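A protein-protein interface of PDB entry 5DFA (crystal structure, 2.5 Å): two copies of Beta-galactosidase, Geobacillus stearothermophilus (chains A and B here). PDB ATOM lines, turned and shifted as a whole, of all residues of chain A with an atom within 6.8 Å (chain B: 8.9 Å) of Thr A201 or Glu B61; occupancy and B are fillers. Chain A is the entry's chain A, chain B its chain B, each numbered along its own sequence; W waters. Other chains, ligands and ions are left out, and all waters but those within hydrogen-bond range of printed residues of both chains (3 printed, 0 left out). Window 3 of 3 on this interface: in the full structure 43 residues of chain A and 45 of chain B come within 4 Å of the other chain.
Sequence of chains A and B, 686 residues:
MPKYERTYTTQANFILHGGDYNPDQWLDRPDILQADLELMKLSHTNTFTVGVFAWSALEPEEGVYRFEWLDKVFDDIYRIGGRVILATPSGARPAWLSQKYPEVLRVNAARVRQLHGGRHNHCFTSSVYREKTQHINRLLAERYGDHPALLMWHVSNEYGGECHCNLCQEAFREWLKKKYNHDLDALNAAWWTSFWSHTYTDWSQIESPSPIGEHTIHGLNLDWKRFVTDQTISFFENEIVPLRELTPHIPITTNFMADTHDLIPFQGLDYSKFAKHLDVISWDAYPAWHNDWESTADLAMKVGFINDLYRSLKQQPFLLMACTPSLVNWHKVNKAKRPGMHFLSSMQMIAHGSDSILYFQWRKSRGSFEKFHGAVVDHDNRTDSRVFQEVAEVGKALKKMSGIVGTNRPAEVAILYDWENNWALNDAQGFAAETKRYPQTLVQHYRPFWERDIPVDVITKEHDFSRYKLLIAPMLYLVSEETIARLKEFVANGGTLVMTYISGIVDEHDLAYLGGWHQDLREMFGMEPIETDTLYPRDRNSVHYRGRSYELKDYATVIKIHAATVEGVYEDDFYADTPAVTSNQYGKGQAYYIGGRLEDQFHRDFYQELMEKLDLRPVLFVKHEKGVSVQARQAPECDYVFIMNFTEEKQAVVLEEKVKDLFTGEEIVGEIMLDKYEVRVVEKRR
Among the printed residues, merely in contact across the chains: Thr A199 with Ser B56, Thr A199 with Ala B95, Thr A201 with Pro B60, Thr A201 with Glu B61, Gln A205 with Ala B95 and Gln A205 with Trp B96.
N of Thr A201 is in hydrogen-bond range of OE1 of Gln A205 (2.9 Å). The side-chain carboxylate (OD2) of Asp A202 sits at hydrogen-bond distance from the side-chain hydroxyl (OG) of Ser A204 (2.6 Å). The side-chain amide oxygen (OE1) of Gln A205 is in hydrogen-bond range of the backbone NH (N) of Asp A202, 3.3 Å away. The backbone carbonyl oxygen (O) of Glu B59 sits at hydrogen-bond distance from the indole nitrogen (NE1) of Trp B96 (2.9 Å). The backbone carbonyl oxygen (O) of Pro B60 sits close to the indole nitrogen (NE1) of Trp B96 (3.3 Å).
No position is printed for both chains.
Water W3 bridges the backbone carbonyl oxygen of Thr A199 (2.6 Å) and the backbone NH of Ala B95 (2.9 Å). Water W2 lies within hydrogen-bond range of the side-chain hydroxyl of Ser B56 (2.7 Å) and the side-chain hydroxyl of Thr A199 (2.8 Å). Water W1 lies within hydrogen-bond range of the backbone carbonyl oxygen of Thr A199 (3.0 Å), the side-chain hydroxyl of Thr A201 (3.0 Å), the backbone NH of Trp B96 (3.1 Å) and the backbone NH of Ala B95 (3.3 Å).
Thr A201 touches just these residues of chain B: Pro B60 (3.4 Å) and Glu B61 (3.5 Å). Of the printed residues of chain A, Glu B61 touches Thr A201 (3.5 Å). Printed residues of chain B within 4 Å of Ser A204: Gln B99. Of the printed residues of chain B, Gln A205 touches Ala B95, Trp B96 and Gln B99. Of the printed residues of chain A, Trp B96 touches Gln A205. Ile B136 touches none of the printed residues of chain A.
Of the 10 printed residues of chain A, 4 touch a printed residue of chain B. Printed residues of chain A that touch a printed residue of chain B: Thr A199, Thr A201, Ser A204 and Gln A205. Printed residues of chain B that touch a printed residue of chain A: Ser B56, Pro B60, Glu B61, Ala B95, Trp B96 and Gln B99.
The side-chain amide nitrogen of Gln B99 is in hydrogen-bond range of the side-chain hydroxyl of Ser A204 (2.7 Å). NE2 of Gln A205 sits close to OE1 of Gln B99, 3.4 Å away.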
ATOM      1  N   LEU A 184      -8.599   6.867  14.316  1.00  0.00           N
ATOM      2  CA  LEU A 184      -9.262   7.114  15.592  1.00  0.00           C
ATOM      3  C   LEU A 184      -8.496   6.473  16.748  1.00  0.00           C
ATOM      4  O   LEU A 184      -8.556   6.949  17.883  1.00  0.00           O
ATOM      5  CB  LEU A 184     -10.699   6.592  15.548  1.00  0.00           C
ATOM      6  CG  LEU A 184     -11.700   7.222  16.516  1.00  0.00           C
ATOM      7  CD1 LEU A 184     -11.629   8.739  16.454  1.00  0.00           C
ATOM      8  CD2 LEU A 184     -13.105   6.740  16.200  1.00  0.00           C
ATOM      9  N   ASN A 188      -7.230   8.478  20.148  1.00  0.00           N
ATOM     10  CA  ASN A 188      -7.565   7.964  21.471  1.00  0.00           C
ATOM     11  C   ASN A 188      -6.326   7.641  22.300  1.00  0.00           C
ATOM     12  O   ASN A 188      -6.324   7.807  23.521  1.00  0.00           O
ATOM     13  CB  ASN A 188      -8.448   6.720  21.348  1.00  0.00           C
ATOM     14  CG  ASN A 188      -9.887   7.056  21.002  1.00  0.00           C
ATOM     15  OD1 ASN A 188     -10.478   7.973  21.575  1.00  0.00           O
ATOM     16  ND2 ASN A 188     -10.457   6.316  20.059  1.00  0.00           N
ATOM     17  N   HIS A 198     -13.671   7.443  28.245  1.00  0.00           N
ATOM     18  CA  HIS A 198     -13.965   8.485  27.262  1.00  0.00           C
ATOM     19  C   HIS A 198     -13.615   8.092  25.827  1.00  0.00           C
ATOM     20  O   HIS A 198     -13.665   8.931  24.927  1.00  0.00           O
ATOM     21  CB  HIS A 198     -13.219   9.774  27.620  1.00  0.00           C
ATOM     22  CG  HIS A 198     -13.756  10.470  28.831  1.00  0.00           C
ATOM     23  ND1 HIS A 198     -12.984  11.299  29.617  1.00  0.00           N
ATOM     24  CD2 HIS A 198     -14.990  10.468  29.388  1.00  0.00           C
ATOM     25  CE1 HIS A 198     -13.718  11.774  30.606  1.00  0.00           C
ATOM     26  NE2 HIS A 198     -14.940  11.285  30.491  1.00  0.00           N
ATOM     27  N   THR A 199     -13.262   6.827  25.618  1.00  0.00           N
ATOM     28  CA  THR A 199     -12.842   6.344  24.301  1.00  0.00           C
ATOM     29  C   THR A 199     -13.873   6.627  23.209  1.00  0.00           C
ATOM     30  O   THR A 199     -15.036   6.241  23.323  1.00  0.00           O
ATOM     31  CB  THR A 199     -12.559   4.830  24.327  1.00  0.00           C
ATOM     32  OG1 THR A 199     -11.470   4.559  25.218  1.00  0.00           O
ATOM     33  CG2 THR A 199     -12.205   4.329  22.936  1.00  0.00           C
ATOM     34  N   TYR A 200     -13.436   7.307  22.153  1.00  0.00           N
ATOM     35  CA  TYR A 200     -14.310   7.636  21.033  1.00  0.00           C
ATOM     36  C   TYR A 200     -14.368   6.493  20.020  1.00  0.00           C
ATOM     37  O   TYR A 200     -13.343   5.903  19.680  1.00  0.00           O
ATOM     38  CB  TYR A 200     -13.841   8.919  20.342  1.00  0.00           C
ATOM     39  CG  TYR A 200     -13.785  10.130  21.246  1.00  0.00           C
ATOM     40  CD1 TYR A 200     -14.947  10.762  21.669  1.00  0.00           C
ATOM     41  CD2 TYR A 200     -12.567  10.651  21.667  1.00  0.00           C
ATOM     42  CE1 TYR A 200     -14.899  11.872  22.491  1.00  0.00           C
ATOM     43  CE2 TYR A 200     -12.509  11.762  22.489  1.00  0.00           C
ATOM     44  CZ  TYR A 200     -13.678  12.368  22.898  1.00  0.00           C
ATOM     45  OH  TYR A 200     -13.628  13.474  23.715  1.00  0.00           O
ATOM     46  N   THR A 201     -15.569   6.192  19.538  1.00  0.00           N
ATOM     47  CA  THR A 201     -15.758   5.124  18.560  1.00  0.00           C
ATOM     48  C   THR A 201     -16.255   5.673  17.227  1.00  0.00           C
ATOM     49  O   THR A 201     -16.389   4.934  16.250  1.00  0.00           O
ATOM     50  CB  THR A 201     -16.747   4.061  19.070  1.00  0.00           C
ATOM     51  OG1 THR A 201     -17.881   4.708  19.660  1.00  0.00           O
ATOM     52  CG2 THR A 201     -16.081   3.176  20.115  1.00  0.00           C
ATOM     53  N   ASP A 202     -16.525   6.972  17.193  1.00  0.00           N
ATOM     54  CA  ASP A 202     -16.911   7.650  15.962  1.00  0.00           C
ATOM     55  C   ASP A 202     -16.495   9.114  16.038  1.00  0.00           C
ATOM     56  O   ASP A 202     -16.527   9.717  17.111  1.00  0.00           O
ATOM     57  CB  ASP A 202     -18.418   7.529  15.720  1.00  0.00           C
ATOM     58  CG  ASP A 202     -18.830   8.026  14.346  1.00  0.00           C
ATOM     59  OD1 ASP A 202     -19.022   7.187  13.442  1.00  0.00           O
ATOM     60  OD2 ASP A 202     -18.959   9.256  14.170  1.00  0.00           O
ATOM     61  N   TRP A 203     -16.104   9.682  14.901  1.00  0.00           N
ATOM     62  CA  TRP A 203     -15.621  11.059  14.860  1.00  0.00           C
ATOM     63  C   TRP A 203     -16.701  12.064  15.257  1.00  0.00           C
ATOM     64  O   TRP A 203     -16.395  13.138  15.773  1.00  0.00           O
ATOM     65  CB  TRP A 203     -15.083  11.396  13.467  1.00  0.00           C
ATOM     66  CG  TRP A 203     -13.858  10.617  13.089  1.00  0.00           C
ATOM     67  CD1 TRP A 203     -13.811   9.469  12.354  1.00  0.00           C
ATOM     68  CD2 TRP A 203     -12.501  10.929  13.431  1.00  0.00           C
ATOM     69  NE1 TRP A 203     -12.511   9.047  12.216  1.00  0.00           N
ATOM     70  CE2 TRP A 203     -11.687   9.927  12.868  1.00  0.00           C
ATOM     71  CE3 TRP A 203     -11.896  11.960  14.158  1.00  0.00           C
ATOM     72  CZ2 TRP A 203     -10.301   9.923  13.008  1.00  0.00           C
ATOM     73  CZ3 TRP A 203     -10.519  11.954  14.298  1.00  0.00           C
ATOM     74  CH2 TRP A 203      -9.737  10.942  13.725  1.00  0.00           C
ATOM     75  N   SER A 204     -17.962  11.707  15.024  1.00  0.00           N
ATOM     76  CA  SER A 204     -19.080  12.594  15.333  1.00  0.00           C
ATOM     77  C   SER A 204     -19.249  12.811  16.835  1.00  0.00           C
ATOM     78  O   SER A 204     -19.891  13.770  17.261  1.00  0.00           O
ATOM     79  CB  SER A 204     -20.378  12.041  14.742  1.00  0.00           C
ATOM     80  OG  SER A 204     -20.691  10.774  15.297  1.00  0.00           O
ATOM     81  N   GLN A 205     -18.675  11.915  17.632  1.00  0.00           N
ATOM     82  CA  GLN A 205     -18.773  12.003  19.083  1.00  0.00           C
ATOM     83  C   GLN A 205     -17.866  13.093  19.644  1.00  0.00           C
ATOM     84  O   GLN A 205     -18.120  13.631  20.723  1.00  0.00           O
ATOM     85  CB  GLN A 205     -18.427  10.657  19.722  1.00  0.00           C
ATOM     86  CG  GLN A 205     -19.412   9.547  19.398  1.00  0.00           C
ATOM     87  CD  GLN A 205     -18.854   8.169  19.696  1.00  0.00           C
ATOM     88  OE1 GLN A 205     -17.714   8.032  20.137  1.00  0.00           O
ATOM     89  NE2 GLN A 205     -19.657   7.141  19.454  1.00  0.00           N
ATOM     90  N   TRP B  55     -16.320   0.662  31.246  1.00  0.00           N
ATOM     91  CA  TRP B  55     -17.504   0.359  30.444  1.00  0.00           C
ATOM     92  C   TRP B  55     -17.190   0.355  28.946  1.00  0.00           C
ATOM     93  O   TRP B  55     -17.605  -0.551  28.227  1.00  0.00           O
ATOM     94  CB  TRP B  55     -18.633   1.350  30.748  1.00  0.00           C
ATOM     95  CG  TRP B  55     -19.998   0.870  30.315  1.00  0.00           C
ATOM     96  CD1 TRP B  55     -20.277  -0.038  29.333  1.00  0.00           C
ATOM     97  CD2 TRP B  55     -21.262   1.262  30.865  1.00  0.00           C
ATOM     98  NE1 TRP B  55     -21.633  -0.227  29.231  1.00  0.00           N
ATOM     99  CE2 TRP B  55     -22.262   0.558  30.161  1.00  0.00           C
ATOM    100  CE3 TRP B  55     -21.648   2.142  31.881  1.00  0.00           C
ATOM    101  CZ2 TRP B  55     -23.617   0.707  30.440  1.00  0.00           C
ATOM    102  CZ3 TRP B  55     -22.996   2.288  32.156  1.00  0.00           C
ATOM    103  CH2 TRP B  55     -23.965   1.574  31.438  1.00  0.00           C
ATOM    104  N   SER B  56     -16.449   1.356  28.480  1.00  0.00           N
ATOM    105  CA  SER B  56     -16.105   1.434  27.063  1.00  0.00           C
ATOM    106  C   SER B  56     -15.166   0.299  26.659  1.00  0.00           C
ATOM    107  O   SER B  56     -15.061  -0.040  25.480  1.00  0.00           O
ATOM    108  CB  SER B  56     -15.468   2.786  26.731  1.00  0.00           C
ATOM    109  OG  SER B  56     -14.180   2.904  27.306  1.00  0.00           O
ATOM    110  N   ALA B  57     -14.490  -0.288  27.641  1.00  0.00           N
ATOM    111  CA  ALA B  57     -13.597  -1.414  27.389  1.00  0.00           C
ATOM    112  C   ALA B  57     -14.357  -2.737  27.427  1.00  0.00           C
ATOM    113  O   ALA B  57     -13.957  -3.712  26.790  1.00  0.00           O
ATOM    114  CB  ALA B  57     -12.460  -1.425  28.399  1.00  0.00           C
ATOM    115  N   LEU B  58     -15.454  -2.765  28.178  1.00  0.00           N
ATOM    116  CA  LEU B  58     -16.288  -3.959  28.273  1.00  0.00           C
ATOM    117  C   LEU B  58     -17.320  -3.998  27.152  1.00  0.00           C
ATOM    118  O   LEU B  58     -17.673  -5.068  26.655  1.00  0.00           O
ATOM    119  CB  LEU B  58     -16.992  -4.018  29.632  1.00  0.00           C
ATOM    120  CG  LEU B  58     -16.113  -4.244  30.863  1.00  0.00           C
ATOM    121  CD1 LEU B  58     -16.942  -4.150  32.134  1.00  0.00           C
ATOM    122  CD2 LEU B  58     -15.412  -5.590  30.778  1.00  0.00           C
ATOM    123  N   GLU B  59     -17.801  -2.823  26.761  1.00  0.00           N
ATOM    124  CA  GLU B  59     -18.813  -2.717  25.717  1.00  0.00           C
ATOM    125  C   GLU B  59     -18.490  -1.560  24.770  1.00  0.00           C
ATOM    126  O   GLU B  59     -19.138  -0.514  24.822  1.00  0.00           O
ATOM    127  CB  GLU B  59     -20.199  -2.532  26.345  1.00  0.00           C
ATOM    128  CG  GLU B  59     -21.362  -2.728  25.388  1.00  0.00           C
ATOM    129  CD  GLU B  59     -22.708  -2.499  26.050  1.00  0.00           C
ATOM    130  OE1 GLU B  59     -22.729  -2.100  27.233  1.00  0.00           O
ATOM    131  OE2 GLU B  59     -23.744  -2.720  25.388  1.00  0.00           O
ATOM    132  N   PRO B  60     -17.480  -1.748  23.903  1.00  0.00           N
ATOM    133  CA  PRO B  60     -16.998  -0.706  22.985  1.00  0.00           C
ATOM    134  C   PRO B  60     -18.084  -0.190  22.043  1.00  0.00           C
ATOM    135  O   PRO B  60     -18.101   0.995  21.712  1.00  0.00           O
ATOM    136  CB  PRO B  60     -15.885  -1.413  22.200  1.00  0.00           C
ATOM    137  CG  PRO B  60     -16.161  -2.869  22.360  1.00  0.00           C
ATOM    138  CD  PRO B  60     -16.743  -3.011  23.728  1.00  0.00           C
ATOM    139  N   GLU B  61     -18.971  -1.081  21.613  1.00  0.00           N
ATOM    140  CA  GLU B  61     -20.157  -0.690  20.863  1.00  0.00           C
ATOM    141  C   GLU B  61     -21.377  -1.275  21.558  1.00  0.00           C
ATOM    142  O   GLU B  61     -21.258  -2.250  22.299  1.00  0.00           O
ATOM    143  CB  GLU B  61     -20.086  -1.164  19.408  1.00  0.00           C
ATOM    144  CG  GLU B  61     -19.095  -0.400  18.540  1.00  0.00           C
ATOM    145  CD  GLU B  61     -17.655  -0.798  18.799  1.00  0.00           C
ATOM    146  OE1 GLU B  61     -17.412  -1.983  19.113  1.00  0.00           O
ATOM    147  OE2 GLU B  61     -16.765   0.072  18.687  1.00  0.00           O
ATOM    148  N   GLU B  62     -22.545  -0.683  21.326  1.00  0.00           N
ATOM    149  CA  GLU B  62     -23.770  -1.156  21.963  1.00  0.00           C
ATOM    150  C   GLU B  62     -24.045  -2.615  21.610  1.00  0.00           C
ATOM    151  O   GLU B  62     -24.235  -2.956  20.443  1.00  0.00           O
ATOM    152  CB  GLU B  62     -24.962  -0.285  21.562  1.00  0.00           C
ATOM    153  CG  GLU B  62     -26.229  -0.587  22.350  1.00  0.00           C
ATOM    154  CD  GLU B  62     -27.380   0.330  21.991  1.00  0.00           C
ATOM    155  OE1 GLU B  62     -27.314   0.987  20.931  1.00  0.00           O
ATOM    156  OE2 GLU B  62     -28.353   0.398  22.772  1.00  0.00           O
ATOM    157  N   GLY B  63     -24.047  -3.473  22.625  1.00  0.00           N
ATOM    158  CA  GLY B  63     -24.322  -4.885  22.431  1.00  0.00           C
ATOM    159  C   GLY B  63     -23.112  -5.697  22.007  1.00  0.00           C
ATOM    160  O   GLY B  63     -23.217  -6.901  21.776  1.00  0.00           O
ATOM    161  N   VAL B  64     -21.962  -5.039  21.897  1.00  0.00           N
ATOM    162  CA  VAL B  64     -20.721  -5.717  21.535  1.00  0.00           C
ATOM    163  C   VAL B  64     -19.800  -5.790  22.747  1.00  0.00           C
ATOM    164  O   VAL B  64     -19.357  -4.764  23.260  1.00  0.00           O
ATOM    165  CB  VAL B  64     -19.998  -5.000  20.380  1.00  0.00           C
ATOM    166  CG1 VAL B  64     -18.728  -5.749  20.006  1.00  0.00           C
ATOM    167  CG2 VAL B  64     -20.922  -4.871  19.177  1.00  0.00           C
ATOM    168  N   TYR B  65     -19.506  -7.004  23.200  1.00  0.00           N
ATOM    169  CA  TYR B  65     -18.831  -7.180  24.480  1.00  0.00           C
ATOM    170  C   TYR B  65     -17.422  -7.760  24.378  1.00  0.00           C
ATOM    171  O   TYR B  65     -17.157  -8.661  23.582  1.00  0.00           O
ATOM    172  CB  TYR B  65     -19.689  -8.057  25.392  1.00  0.00           C
ATOM    173  CG  TYR B  65     -21.022  -7.427  25.729  1.00  0.00           C
ATOM    174  CD1 TYR B  65     -21.102  -6.376  26.633  1.00  0.00           C
ATOM    175  CD2 TYR B  65     -22.195  -7.872  25.135  1.00  0.00           C
ATOM    176  CE1 TYR B  65     -22.314  -5.789  26.942  1.00  0.00           C
ATOM    177  CE2 TYR B  65     -23.415  -7.292  25.439  1.00  0.00           C
ATOM    178  CZ  TYR B  65     -23.466  -6.250  26.342  1.00  0.00           C
ATOM    179  OH  TYR B  65     -24.674  -5.668  26.652  1.00  0.00           O
ATOM    180  N   ARG B  66     -16.527  -7.225  25.203  1.00  0.00           N
ATOM    181  CA  ARG B  66     -15.144  -7.680  25.276  1.00  0.00           C
ATOM    182  C   ARG B  66     -14.753  -7.962  26.725  1.00  0.00           C
ATOM    183  O   ARG B  66     -14.272  -7.073  27.429  1.00  0.00           O
ATOM    184  CB  ARG B  66     -14.200  -6.637  24.670  1.00  0.00           C
ATOM    185  CG  ARG B  66     -14.433  -6.355  23.194  1.00  0.00           C
ATOM    186  CD  ARG B  66     -13.852  -7.455  22.318  1.00  0.00           C
ATOM    187  NE  ARG B  66     -14.081  -7.203  20.899  1.00  0.00           N
ATOM    188  CZ  ARG B  66     -15.096  -7.707  20.204  1.00  0.00           C
ATOM    189  NH1 ARG B  66     -15.981  -8.496  20.798  1.00  0.00           N
ATOM    190  NH2 ARG B  66     -15.225  -7.423  18.915  1.00  0.00           N
ATOM    191  N   PRO B  94     -20.018   5.273  28.291  1.00  0.00           N
ATOM    192  CA  PRO B  94     -19.297   5.328  27.016  1.00  0.00           C
ATOM    193  C   PRO B  94     -19.861   6.421  26.114  1.00  0.00           C
ATOM    194  O   PRO B  94     -21.018   6.806  26.277  1.00  0.00           O
ATOM    195  CB  PRO B  94     -19.529   3.938  26.414  1.00  0.00           C
ATOM    196  CG  PRO B  94     -19.887   3.070  27.574  1.00  0.00           C
ATOM    197  CD  PRO B  94     -20.641   3.958  28.514  1.00  0.00           C
ATOM    198  N   ALA B  95     -19.054   6.907  25.176  1.00  0.00           N
ATOM    199  CA  ALA B  95     -19.466   8.005  24.307  1.00  0.00           C
ATOM    200  C   ALA B  95     -20.662   7.632  23.431  1.00  0.00           C
ATOM    201  O   ALA B  95     -21.515   8.475  23.154  1.00  0.00           O
ATOM    202  CB  ALA B  95     -18.300   8.456  23.440  1.00  0.00           C
ATOM    203  N   TRP B  96     -20.725   6.374  23.003  1.00  0.00           N
ATOM    204  CA  TRP B  96     -21.813   5.929  22.136  1.00  0.00           C
ATOM    205  C   TRP B  96     -23.149   5.937  22.871  1.00  0.00           C
ATOM    206  O   TRP B  96     -24.204   6.066  22.251  1.00  0.00           O
ATOM    207  CB  TRP B  96     -21.530   4.531  21.564  1.00  0.00           C
ATOM    208  CG  TRP B  96     -21.327   3.443  22.591  1.00  0.00           C
ATOM    209  CD1 TRP B  96     -20.134   2.926  23.006  1.00  0.00           C
ATOM    210  CD2 TRP B  96     -22.345   2.729  23.309  1.00  0.00           C
ATOM    211  NE1 TRP B  96     -20.344   1.942  23.942  1.00  0.00           N
ATOM    212  CE2 TRP B  96     -21.692   1.804  24.147  1.00  0.00           C
ATOM    213  CE3 TRP B  96     -23.742   2.784  23.328  1.00  0.00           C
ATOM    214  CZ2 TRP B  96     -22.387   0.944  24.996  1.00  0.00           C
ATOM    215  CZ3 TRP B  96     -24.430   1.934  24.175  1.00  0.00           C
ATOM    216  CH2 TRP B  96     -23.753   1.024  24.994  1.00  0.00           C
ATOM    217  N   LEU B  97     -23.100   5.803  24.192  1.00  0.00           N
ATOM    218  CA  LEU B  97     -24.316   5.776  24.998  1.00  0.00           C
ATOM    219  C   LEU B  97     -24.916   7.173  25.116  1.00  0.00           C
ATOM    220  O   LEU B  97     -26.125   7.353  24.965  1.00  0.00           O
ATOM    221  CB  LEU B  97     -24.027   5.194  26.384  1.00  0.00           C
ATOM    222  CG  LEU B  97     -25.201   4.543  27.124  1.00  0.00           C
ATOM    223  CD1 LEU B  97     -24.704   3.427  28.027  1.00  0.00           C
ATOM    224  CD2 LEU B  97     -25.985   5.570  27.930  1.00  0.00           C
ATOM    225  N   GLN B  99     -24.323   9.688  23.076  1.00  0.00           N
ATOM    226  CA  GLN B  99     -24.682  10.149  21.740  1.00  0.00           C
ATOM    227  C   GLN B  99     -26.043   9.611  21.308  1.00  0.00           C
ATOM    228  O   GLN B  99     -26.852  10.338  20.733  1.00  0.00           O
ATOM    229  CB  GLN B  99     -23.615   9.739  20.722  1.00  0.00           C
ATOM    230  CG  GLN B  99     -23.800  10.370  19.350  1.00  0.00           C
ATOM    231  CD  GLN B  99     -22.809   9.853  18.327  1.00  0.00           C
ATOM    232  OE1 GLN B  99     -22.456   8.673  18.328  1.00  0.00           O
ATOM    233  NE2 GLN B  99     -22.356  10.733  17.443  1.00  0.00           N
ATOM    234  N   LYS B 100     -26.293   8.337  21.594  1.00  0.00           N
ATOM    235  CA  LYS B 100     -27.523   7.688  21.156  1.00  0.00           C
ATOM    236  C   LYS B 100     -28.682   7.928  22.122  1.00  0.00           C
ATOM    237  O   LYS B 100     -29.827   8.077  21.697  1.00  0.00           O
ATOM    238  CB  LYS B 100     -27.298   6.184  20.976  1.00  0.00           C
ATOM    239  CG  LYS B 100     -28.505   5.448  20.418  1.00  0.00           C
ATOM    240  CD  LYS B 100     -28.151   4.038  19.980  1.00  0.00           C
ATOM    241  CE  LYS B 100     -29.389   3.285  19.517  1.00  0.00           C
ATOM    242  NZ  LYS B 100     -29.062   1.915  19.037  1.00  0.00           N
ATOM    243  N   LYS B 132     -29.536   0.027  31.279  1.00  0.00           N
ATOM    244  CA  LYS B 132     -28.191  -0.271  30.796  1.00  0.00           C
ATOM    245  C   LYS B 132     -27.260  -0.711  31.920  1.00  0.00           C
ATOM    246  O   LYS B 132     -26.552  -1.710  31.792  1.00  0.00           O
ATOM    247  CB  LYS B 132     -27.597   0.946  30.085  1.00  0.00           C
ATOM    248  CG  LYS B 132     -28.274   1.307  28.773  1.00  0.00           C
ATOM    249  CD  LYS B 132     -28.050   0.244  27.715  1.00  0.00           C
ATOM    250  CE  LYS B 132     -28.449   0.757  26.340  1.00  0.00           C
ATOM    251  NZ  LYS B 132     -28.435  -0.319  25.313  1.00  0.00           N
ATOM    252  N   ILE B 136     -25.494  -4.540  32.337  1.00  0.00           N
ATOM    253  CA  ILE B 136     -24.053  -4.769  32.321  1.00  0.00           C
ATOM    254  C   ILE B 136     -23.601  -5.335  33.669  1.00  0.00           C
ATOM    255  O   ILE B 136     -22.660  -6.126  33.733  1.00  0.00           O
ATOM    256  CB  ILE B 136     -23.263  -3.474  31.979  1.00  0.00           C
ATOM    257  CG1 ILE B 136     -21.763  -3.763  31.881  1.00  0.00           C
ATOM    258  CG2 ILE B 136     -23.530  -2.377  32.993  1.00  0.00           C
ATOM    259  CD1 ILE B 136     -21.388  -4.656  30.721  1.00  0.00           C
HETATM  260  O   HOH W   1     -17.781   5.361  22.566  1.00  0.00           O
HETATM  261  O   HOH W   2     -12.136   1.939  25.816  1.00  0.00           O
HETATM  262  O   HOH W   3     -16.356   6.087  25.592  1.00  0.00           O
